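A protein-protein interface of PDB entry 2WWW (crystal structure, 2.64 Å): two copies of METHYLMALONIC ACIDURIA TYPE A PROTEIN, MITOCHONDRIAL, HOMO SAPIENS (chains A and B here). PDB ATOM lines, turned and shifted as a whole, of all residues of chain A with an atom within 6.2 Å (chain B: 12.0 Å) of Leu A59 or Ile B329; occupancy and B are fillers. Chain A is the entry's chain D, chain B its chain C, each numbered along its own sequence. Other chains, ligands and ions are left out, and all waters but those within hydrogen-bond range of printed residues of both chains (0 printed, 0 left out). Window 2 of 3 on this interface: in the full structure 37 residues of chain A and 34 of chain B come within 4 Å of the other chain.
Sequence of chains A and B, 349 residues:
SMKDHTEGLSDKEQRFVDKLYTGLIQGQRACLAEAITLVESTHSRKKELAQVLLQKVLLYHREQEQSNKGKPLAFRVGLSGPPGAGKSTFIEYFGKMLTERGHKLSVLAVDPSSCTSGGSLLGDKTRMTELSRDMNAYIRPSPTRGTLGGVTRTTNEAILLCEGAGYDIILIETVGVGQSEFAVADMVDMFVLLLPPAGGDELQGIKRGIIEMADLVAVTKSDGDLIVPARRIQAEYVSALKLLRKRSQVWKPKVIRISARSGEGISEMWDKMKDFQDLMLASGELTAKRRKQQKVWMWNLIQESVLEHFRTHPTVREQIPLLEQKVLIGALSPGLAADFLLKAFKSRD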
ATOM      1  N   TYR A  21       7.734 -16.603 -19.447  1.00  0.00           N
ATOM      2  CA  TYR A  21       7.566 -17.637 -18.440  1.00  0.00           C
ATOM      3  C   TYR A  21       6.510 -18.698 -18.856  1.00  0.00           C
ATOM      4  O   TYR A  21       6.774 -19.916 -18.807  1.00  0.00           O
ATOM      5  CB  TYR A  21       7.167 -16.988 -17.109  1.00  0.00           C
ATOM      6  CG  TYR A  21       6.830 -17.990 -16.026  1.00  0.00           C
ATOM      7  CD1 TYR A  21       7.832 -18.734 -15.398  1.00  0.00           C
ATOM      8  CD2 TYR A  21       5.508 -18.235 -15.662  1.00  0.00           C
ATOM      9  CE1 TYR A  21       7.524 -19.706 -14.447  1.00  0.00           C
ATOM     10  CE2 TYR A  21       5.189 -19.211 -14.717  1.00  0.00           C
ATOM     11  CZ  TYR A  21       6.201 -19.938 -14.106  1.00  0.00           C
ATOM     12  OH  TYR A  21       5.870 -20.891 -13.169  1.00  0.00           O
ATOM     13  N   LEU A  54      14.221 -16.196 -13.858  1.00  0.00           N
ATOM     14  CA  LEU A  54      14.885 -17.351 -13.249  1.00  0.00           C
ATOM     15  C   LEU A  54      14.316 -17.694 -11.898  1.00  0.00           C
ATOM     16  O   LEU A  54      14.238 -18.874 -11.599  1.00  0.00           O
ATOM     17  CB  LEU A  54      16.397 -17.110 -13.133  1.00  0.00           C
ATOM     18  CG  LEU A  54      17.158 -17.096 -14.445  1.00  0.00           C
ATOM     19  CD1 LEU A  54      18.487 -16.347 -14.322  1.00  0.00           C
ATOM     20  CD2 LEU A  54      17.200 -18.511 -15.108  1.00  0.00           C
ATOM     21  N   GLN A  55      13.931 -16.684 -11.074  1.00  0.00           N
ATOM     22  CA  GLN A  55      13.294 -16.925  -9.791  1.00  0.00           C
ATOM     23  C   GLN A  55      11.917 -17.566  -9.944  1.00  0.00           C
ATOM     24  O   GLN A  55      11.557 -18.477  -9.153  1.00  0.00           O
ATOM     25  CB  GLN A  55      13.197 -15.660  -8.969  1.00  0.00           C
ATOM     26  CG  GLN A  55      13.087 -15.985  -7.471  1.00  0.00           C
ATOM     27  CD  GLN A  55      13.146 -14.762  -6.599  1.00  0.00           C
ATOM     28  OE1 GLN A  55      13.802 -13.750  -6.929  1.00  0.00           O
ATOM     29  NE2 GLN A  55      12.475 -14.837  -5.439  1.00  0.00           N
ATOM     30  N   LYS A  56      11.147 -17.118 -10.949  1.00  0.00           N
ATOM     31  CA  LYS A  56       9.853 -17.755 -11.251  1.00  0.00           C
ATOM     32  C   LYS A  56      10.073 -19.232 -11.683  1.00  0.00           C
ATOM     33  O   LYS A  56       9.392 -20.124 -11.189  1.00  0.00           O
ATOM     34  CB  LYS A  56       9.098 -16.975 -12.334  1.00  0.00           C
ATOM     35  CG  LYS A  56       8.605 -15.577 -11.917  1.00  0.00           C
ATOM     36  CD  LYS A  56       8.024 -14.848 -13.100  1.00  0.00           C
ATOM     37  CE  LYS A  56       6.718 -14.185 -12.746  1.00  0.00           C
ATOM     38  NZ  LYS A  56       6.904 -12.785 -12.250  1.00  0.00           N
ATOM     39  N   VAL A  57      11.070 -19.500 -12.554  1.00  0.00           N
ATOM     40  CA  VAL A  57      11.411 -20.871 -13.002  1.00  0.00           C
ATOM     41  C   VAL A  57      11.966 -21.745 -11.858  1.00  0.00           C
ATOM     42  O   VAL A  57      11.702 -22.943 -11.833  1.00  0.00           O
ATOM     43  CB  VAL A  57      12.269 -20.893 -14.299  1.00  0.00           C
ATOM     44  CG1 VAL A  57      12.588 -22.312 -14.736  1.00  0.00           C
ATOM     45  CG2 VAL A  57      11.556 -20.155 -15.419  1.00  0.00           C
ATOM     46  N   LEU A  58      12.697 -21.164 -10.909  1.00  0.00           N
ATOM     47  CA  LEU A  58      13.217 -21.879  -9.737  1.00  0.00           C
ATOM     48  C   LEU A  58      12.069 -22.391  -8.867  1.00  0.00           C
ATOM     49  O   LEU A  58      12.107 -23.541  -8.413  1.00  0.00           O
ATOM     50  CB  LEU A  58      14.172 -20.985  -8.900  1.00  0.00           C
ATOM     51  CG  LEU A  58      15.665 -21.021  -9.335  1.00  0.00           C
ATOM     52  CD1 LEU A  58      16.551 -19.912  -8.611  1.00  0.00           C
ATOM     53  CD2 LEU A  58      16.303 -22.448  -9.225  1.00  0.00           C
ATOM     54  N   LEU A  59      11.035 -21.559  -8.662  1.00  0.00           N
ATOM     55  CA  LEU A  59       9.836 -21.929  -7.906  1.00  0.00           C
ATOM     56  C   LEU A  59       9.029 -23.013  -8.614  1.00  0.00           C
ATOM     57  O   LEU A  59       8.525 -23.913  -7.960  1.00  0.00           O
ATOM     58  CB  LEU A  59       8.939 -20.725  -7.691  1.00  0.00           C
ATOM     59  CG  LEU A  59       9.455 -19.654  -6.771  1.00  0.00           C
ATOM     60  CD1 LEU A  59       8.786 -18.351  -7.059  1.00  0.00           C
ATOM     61  CD2 LEU A  59       9.278 -20.058  -5.325  1.00  0.00           C
ATOM     62  N   TYR A  60       8.876 -22.912  -9.937  1.00  0.00           N
ATOM     63  CA  TYR A  60       8.127 -23.894 -10.734  1.00  0.00           C
ATOM     64  C   TYR A  60       8.871 -25.211 -10.792  1.00  0.00           C
ATOM     65  O   TYR A  60       8.252 -26.264 -10.642  1.00  0.00           O
ATOM     66  CB  TYR A  60       7.859 -23.347 -12.135  1.00  0.00           C
ATOM     67  CG  TYR A  60       7.173 -24.322 -13.057  1.00  0.00           C
ATOM     68  CD1 TYR A  60       5.810 -24.587 -12.938  1.00  0.00           C
ATOM     69  CD2 TYR A  60       7.872 -24.954 -14.076  1.00  0.00           C
ATOM     70  CE1 TYR A  60       5.159 -25.465 -13.811  1.00  0.00           C
ATOM     71  CE2 TYR A  60       7.240 -25.860 -14.940  1.00  0.00           C
ATOM     72  CZ  TYR A  60       5.883 -26.109 -14.804  1.00  0.00           C
ATOM     73  OH  TYR A  60       5.280 -27.007 -15.651  1.00  0.00           O
ATOM     74  N   HIS A  61      10.193 -25.163 -10.982  1.00  0.00           N
ATOM     75  CA  HIS A  61      11.074 -26.322 -11.009  1.00  0.00           C
ATOM     76  C   HIS A  61      10.893 -27.135  -9.725  1.00  0.00           C
ATOM     77  O   HIS A  61      10.799 -28.370  -9.794  1.00  0.00           O
ATOM     78  CB  HIS A  61      12.523 -25.844 -11.136  1.00  0.00           C
ATOM     79  CG  HIS A  61      13.507 -26.911 -11.474  1.00  0.00           C
ATOM     80  ND1 HIS A  61      14.051 -27.745 -10.496  1.00  0.00           N
ATOM     81  CD2 HIS A  61      14.031 -27.248 -12.677  1.00  0.00           C
ATOM     82  CE1 HIS A  61      14.905 -28.536 -11.133  1.00  0.00           C
ATOM     83  NE2 HIS A  61      14.936 -28.274 -12.444  1.00  0.00           N
ATOM     84  N   ARG A  62      10.795 -26.439  -8.552  1.00  0.00           N
ATOM     85  CA  ARG A  62      10.563 -27.045  -7.247  1.00  0.00           C
ATOM     86  C   ARG A  62       9.193 -27.681  -7.159  1.00  0.00           C
ATOM     87  O   ARG A  62       9.084 -28.780  -6.642  1.00  0.00           O
ATOM     88  CB  ARG A  62      10.794 -26.046  -6.109  1.00  0.00           C
ATOM     89  CG  ARG A  62      11.123 -26.807  -4.828  1.00  0.00           C
ATOM     90  CD  ARG A  62      11.507 -25.953  -3.653  1.00  0.00           C
ATOM     91  NE  ARG A  62      11.541 -26.743  -2.406  1.00  0.00           N
ATOM     92  CZ  ARG A  62      12.519 -27.589  -2.057  1.00  0.00           C
ATOM     93  NH1 ARG A  62      13.569 -27.781  -2.857  1.00  0.00           N
ATOM     94  NH2 ARG A  62      12.452 -28.251  -0.903  1.00  0.00           N
ATOM     95  N   GLU A  63       8.158 -27.041  -7.718  1.00  0.00           N
ATOM     96  CA  GLU A  63       6.789 -27.571  -7.778  1.00  0.00           C
ATOM     97  C   GLU A  63       6.801 -28.870  -8.581  1.00  0.00           C
ATOM     98  O   GLU A  63       6.235 -29.864  -8.118  1.00  0.00           O
ATOM     99  CB  GLU A  63       5.805 -26.591  -8.470  1.00  0.00           C
ATOM    100  CG  GLU A  63       5.259 -25.419  -7.669  1.00  0.00           C
ATOM    101  CD  GLU A  63       4.410 -24.447  -8.495  1.00  0.00           C
ATOM    102  OE1 GLU A  63       3.463 -24.893  -9.188  1.00  0.00           O
ATOM    103  OE2 GLU A  63       4.703 -23.229  -8.453  1.00  0.00           O
ATOM    104  N   GLN A  64       7.441 -28.854  -9.782  1.00  0.00           N
ATOM    105  CA  GLN A  64       7.582 -29.988 -10.694  1.00  0.00           C
ATOM    106  C   GLN A  64       8.215 -31.194  -9.975  1.00  0.00           C
ATOM    107  O   GLN A  64       7.676 -32.332 -10.087  1.00  0.00           O
ATOM    108  CB  GLN A  64       8.501 -29.650 -11.866  1.00  0.00           C
ATOM    109  CG  GLN A  64       8.008 -28.679 -12.926  1.00  0.00           C
ATOM    110  CD  GLN A  64       9.045 -28.591 -14.062  1.00  0.00           C
ATOM    111  OE1 GLN A  64      10.223 -28.212 -13.863  1.00  0.00           O
ATOM    112  NE2 GLN A  64       8.631 -28.962 -15.282  1.00  0.00           N
ATOM    113  N   ILE B 320      25.687 -18.390   5.299  1.00  0.00           N
ATOM    114  CA  ILE B 320      25.837 -18.870   3.917  1.00  0.00           C
ATOM    115  C   ILE B 320      25.025 -20.161   3.563  1.00  0.00           C
ATOM    116  O   ILE B 320      24.288 -20.110   2.575  1.00  0.00           O
ATOM    117  CB  ILE B 320      27.319 -18.895   3.457  1.00  0.00           C
ATOM    118  CG1 ILE B 320      27.844 -17.459   3.239  1.00  0.00           C
ATOM    119  CG2 ILE B 320      27.486 -19.710   2.205  1.00  0.00           C
ATOM    120  CD1 ILE B 320      29.420 -17.298   3.101  1.00  0.00           C
ATOM    121  N   PRO B 321      25.071 -21.265   4.345  1.00  0.00           N
ATOM    122  CA  PRO B 321      24.302 -22.461   3.969  1.00  0.00           C
ATOM    123  C   PRO B 321      22.812 -22.201   3.827  1.00  0.00           C
ATOM    124  O   PRO B 321      22.250 -22.516   2.791  1.00  0.00           O
ATOM    125  CB  PRO B 321      24.621 -23.467   5.089  1.00  0.00           C
ATOM    126  CG  PRO B 321      25.867 -23.065   5.623  1.00  0.00           C
ATOM    127  CD  PRO B 321      25.857 -21.545   5.558  1.00  0.00           C
ATOM    128  N   LEU B 322      22.200 -21.592   4.830  1.00  0.00           N
ATOM    129  CA  LEU B 322      20.782 -21.253   4.840  1.00  0.00           C
ATOM    130  C   LEU B 322      20.398 -20.365   3.650  1.00  0.00           C
ATOM    131  O   LEU B 322      19.365 -20.574   3.024  1.00  0.00           O
ATOM    132  CB  LEU B 322      20.463 -20.519   6.156  1.00  0.00           C
ATOM    133  CG  LEU B 322      18.990 -20.192   6.414  1.00  0.00           C
ATOM    134  CD1 LEU B 322      18.032 -21.412   6.105  1.00  0.00           C
ATOM    135  CD2 LEU B 322      18.819 -19.715   7.816  1.00  0.00           C
ATOM    136  N   LEU B 323      21.252 -19.392   3.346  1.00  0.00           N
ATOM    137  CA  LEU B 323      21.064 -18.428   2.292  1.00  0.00           C
ATOM    138  C   LEU B 323      21.076 -19.032   0.888  1.00  0.00           C
ATOM    139  O   LEU B 323      20.197 -18.693   0.090  1.00  0.00           O
ATOM    140  CB  LEU B 323      22.063 -17.287   2.476  1.00  0.00           C
ATOM    141  CG  LEU B 323      21.528 -15.967   3.020  1.00  0.00           C
ATOM    142  CD1 LEU B 323      20.738 -16.154   4.270  1.00  0.00           C
ATOM    143  CD2 LEU B 323      22.661 -14.984   3.239  1.00  0.00           C
ATOM    144  N   GLU B 324      22.014 -19.949   0.608  1.00  0.00           N
ATOM    145  CA  GLU B 324      22.131 -20.709  -0.638  1.00  0.00           C
ATOM    146  C   GLU B 324      20.855 -21.555  -0.841  1.00  0.00           C
ATOM    147  O   GLU B 324      20.351 -21.646  -1.960  1.00  0.00           O
ATOM    148  CB  GLU B 324      23.346 -21.634  -0.569  1.00  0.00           C
ATOM    149  CG  GLU B 324      24.689 -20.918  -0.639  1.00  0.00           C
ATOM    150  CD  GLU B 324      25.896 -21.806  -0.352  1.00  0.00           C
ATOM    151  OE1 GLU B 324      25.725 -22.865   0.291  1.00  0.00           O
ATOM    152  OE2 GLU B 324      27.024 -21.434  -0.747  1.00  0.00           O
ATOM    153  N   GLN B 325      20.312 -22.123   0.227  1.00  0.00           N
ATOM    154  CA  GLN B 325      19.082 -22.916   0.139  1.00  0.00           C
ATOM    155  C   GLN B 325      17.935 -22.033  -0.321  1.00  0.00           C
ATOM    156  O   GLN B 325      17.332 -22.345  -1.353  1.00  0.00           O
ATOM    157  CB  GLN B 325      18.743 -23.690   1.451  1.00  0.00           C
ATOM    158  N   LYS B 326      17.704 -20.893   0.389  1.00  0.00           N
ATOM    159  CA  LYS B 326      16.682 -19.882   0.091  1.00  0.00           C
ATOM    160  C   LYS B 326      16.726 -19.384  -1.365  1.00  0.00           C
ATOM    161  O   LYS B 326      15.679 -19.234  -1.971  1.00  0.00           O
ATOM    162  CB  LYS B 326      16.789 -18.676   1.062  1.00  0.00           C
ATOM    163  CG  LYS B 326      16.545 -19.004   2.529  1.00  0.00           C
ATOM    164  CD  LYS B 326      15.095 -19.314   2.843  1.00  0.00           C
ATOM    165  CE  LYS B 326      14.934 -19.947   4.206  1.00  0.00           C
ATOM    166  NZ  LYS B 326      15.200 -18.976   5.296  1.00  0.00           N
ATOM    167  N   VAL B 327      17.920 -19.137  -1.916  1.00  0.00           N
ATOM    168  CA  VAL B 327      18.083 -18.648  -3.290  1.00  0.00           C
ATOM    169  C   VAL B 327      17.596 -19.707  -4.305  1.00  0.00           C
ATOM    170  O   VAL B 327      16.756 -19.410  -5.153  1.00  0.00           O
ATOM    171  CB  VAL B 327      19.507 -18.096  -3.601  1.00  0.00           C
ATOM    172  CG1 VAL B 327      19.649 -17.646  -5.059  1.00  0.00           C
ATOM    173  CG2 VAL B 327      19.877 -16.959  -2.668  1.00  0.00           C
ATOM    174  N   LEU B 328      18.074 -20.938  -4.162  1.00  0.00           N
ATOM    175  CA  LEU B 328      17.795 -22.087  -5.010  1.00  0.00           C
ATOM    176  C   LEU B 328      16.335 -22.520  -4.999  1.00  0.00           C
ATOM    177  O   LEU B 328      15.828 -22.943  -6.030  1.00  0.00           O
ATOM    178  CB  LEU B 328      18.726 -23.220  -4.586  1.00  0.00           C
ATOM    179  CG  LEU B 328      18.708 -24.444  -5.456  1.00  0.00           C
ATOM    180  CD1 LEU B 328      19.679 -24.280  -6.691  1.00  0.00           C
ATOM    181  CD2 LEU B 328      18.939 -25.646  -4.614  1.00  0.00           C
ATOM    182  N   ILE B 329      15.688 -22.465  -3.856  1.00  0.00           N
ATOM    183  CA  ILE B 329      14.268 -22.785  -3.628  1.00  0.00           C
ATOM    184  C   ILE B 329      13.354 -21.635  -4.257  1.00  0.00           C
ATOM    185  O   ILE B 329      12.119 -21.749  -4.327  1.00  0.00           O
ATOM    186  CB  ILE B 329      14.163 -22.931  -2.064  1.00  0.00           C
ATOM    187  CG1 ILE B 329      14.220 -24.364  -1.634  1.00  0.00           C
ATOM    188  CG2 ILE B 329      13.079 -22.149  -1.306  1.00  0.00           C
ATOM    189  CD1 ILE B 329      15.569 -25.127  -1.865  1.00  0.00           C
ATOM    190  N   GLY B 330      14.012 -20.553  -4.694  1.00  0.00           N
ATOM    191  CA  GLY B 330      13.401 -19.378  -5.292  1.00  0.00           C
ATOM    192  C   GLY B 330      12.758 -18.453  -4.295  1.00  0.00           C
ATOM    193  O   GLY B 330      11.921 -17.648  -4.691  1.00  0.00           O
ATOM    194  N   ALA B 331      13.112 -18.576  -2.987  1.00  0.00           N
ATOM    195  CA  ALA B 331      12.573 -17.725  -1.889  1.00  0.00           C
ATOM    196  C   ALA B 331      13.296 -16.397  -1.776  1.00  0.00           C
ATOM    197  O   ALA B 331      12.825 -15.505  -1.106  1.00  0.00           O
ATOM    198  CB  ALA B 331      12.674 -18.459  -0.557  1.00  0.00           C
ATOM    199  N   LEU B 332      14.450 -16.284  -2.385  1.00  0.00           N
ATOM    200  CA  LEU B 332      15.305 -15.107  -2.285  1.00  0.00           C
ATOM    201  C   LEU B 332      16.169 -14.923  -3.563  1.00  0.00           C
ATOM    202  O   LEU B 332      16.536 -15.898  -4.222  1.00  0.00           O
ATOM    203  CB  LEU B 332      16.207 -15.353  -1.054  1.00  0.00           C
ATOM    204  CG  LEU B 332      16.922 -14.223  -0.370  1.00  0.00           C
ATOM    205  CD1 LEU B 332      15.937 -13.162   0.132  1.00  0.00           C
ATOM    206  CD2 LEU B 332      17.692 -14.774   0.766  1.00  0.00           C
ATOM    207  N   SER B 333      16.472 -13.679  -3.894  1.00  0.00           N
ATOM    208  CA  SER B 333      17.298 -13.328  -5.034  1.00  0.00           C
ATOM    209  C   SER B 333      18.772 -13.225  -4.564  1.00  0.00           C
ATOM    210  O   SER B 333      19.025 -12.866  -3.417  1.00  0.00           O
ATOM    211  CB  SER B 333      16.857 -11.982  -5.593  1.00  0.00           C
ATOM    212  OG  SER B 333      16.947 -10.977  -4.591  1.00  0.00           O
ATOM    213  N   PRO B 334      19.775 -13.458  -5.438  1.00  0.00           N
ATOM    214  CA  PRO B 334      21.176 -13.301  -4.987  1.00  0.00           C
ATOM    215  C   PRO B 334      21.501 -11.919  -4.391  1.00  0.00           C
ATOM    216  O   PRO B 334      22.277 -11.883  -3.411  1.00  0.00           O
ATOM    217  CB  PRO B 334      22.005 -13.599  -6.264  1.00  0.00           C
ATOM    218  CG  PRO B 334      21.098 -14.405  -7.115  1.00  0.00           C
ATOM    219  CD  PRO B 334      19.713 -13.876  -6.858  1.00  0.00           C
ATOM    220  N   ALA B 337      20.167 -11.554  -0.852  1.00  0.00           N
ATOM    221  CA  ALA B 337      20.978 -12.476  -0.053  1.00  0.00           C
ATOM    222  C   ALA B 337      22.327 -11.823   0.194  1.00  0.00           C
ATOM    223  O   ALA B 337      22.836 -11.902   1.302  1.00  0.00           O
ATOM    224  CB  ALA B 337      21.148 -13.782  -0.809  1.00  0.00           C
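NE2 of Gln A55 sits at hydrogen-bond distance from O of Gly B330 (3.0 Å).
The backbone carbonyl oxygen (O) of Lys B326 sits at hydrogen-bond distance from the backbone NH (N) of Leu B332 (3.2 Å).
Leu B332 touches Gln A55. Gln A55 touches Ser B333. CD1 of Leu A58 touches O of Val B327, at 3.5 Å. O of Leu B328 touches CD2 of Leu A58, at 3.3 Å. O of Ile B329 touches CD2 of Leu A59, at 3.5 Å. Gly B330 touches Leu A59. Ile B329 touches Arg A62 (CD1 to NH1, 3.5 Å).
Ile B329 touches two residues of chain A. Of chain B, only Gly B330 (3.0 Å), Leu B332 (3.9 Å) and Ser B333 (3.8 Å) come within 4 Å of Gln A55. No residue of chain B comes within 4 Å of Val A57. Of chain B, only Val B327 and Leu B328 come within 4 Å of Leu A58. Glu A63 touches none of the printed residues of chain B. Printed residues of chain A within 4 Å of Leu B328: Leu A58 (3.3 Å). Printed residues of chain A within 4 Å of Val B327: Leu A58 (3.5 Å). Printed residues of chain A within 4 Å of Gly B330: Gln A55 and Leu A59. Of the printed residues of chain A, Ser B333 touches Gln A55. Printed residues of chain A within 4 Å of Leu B332: Gln A55. Ile B320 touches none of the printed residues of chain A. Leu A54 touches none of the printed residues of chain B. The nearest residue of chain B that does not touch Leu A59 is Ala B331 (4.7 Å). The nearest residue of chain A that does not touch Ile B329 is Leu A58 (4.5 Å). The nearest printed residue of chain A that does not touch Leu B328 is Leu A59 (5.6 Å).
Of the 12 printed residues of chain A, 4 touch a printed residue of chain B. Hydrophobic or aromatic side chains of chain A within 4 Å of the printed part of chain B: Leu A58 and Leu A59. Hydrophobic or aromatic side chains of chain B that line the printed part of chain A: Ile B329. Among the printed residues, 8 pairs touch across the chains.
No position is printed for both chains.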
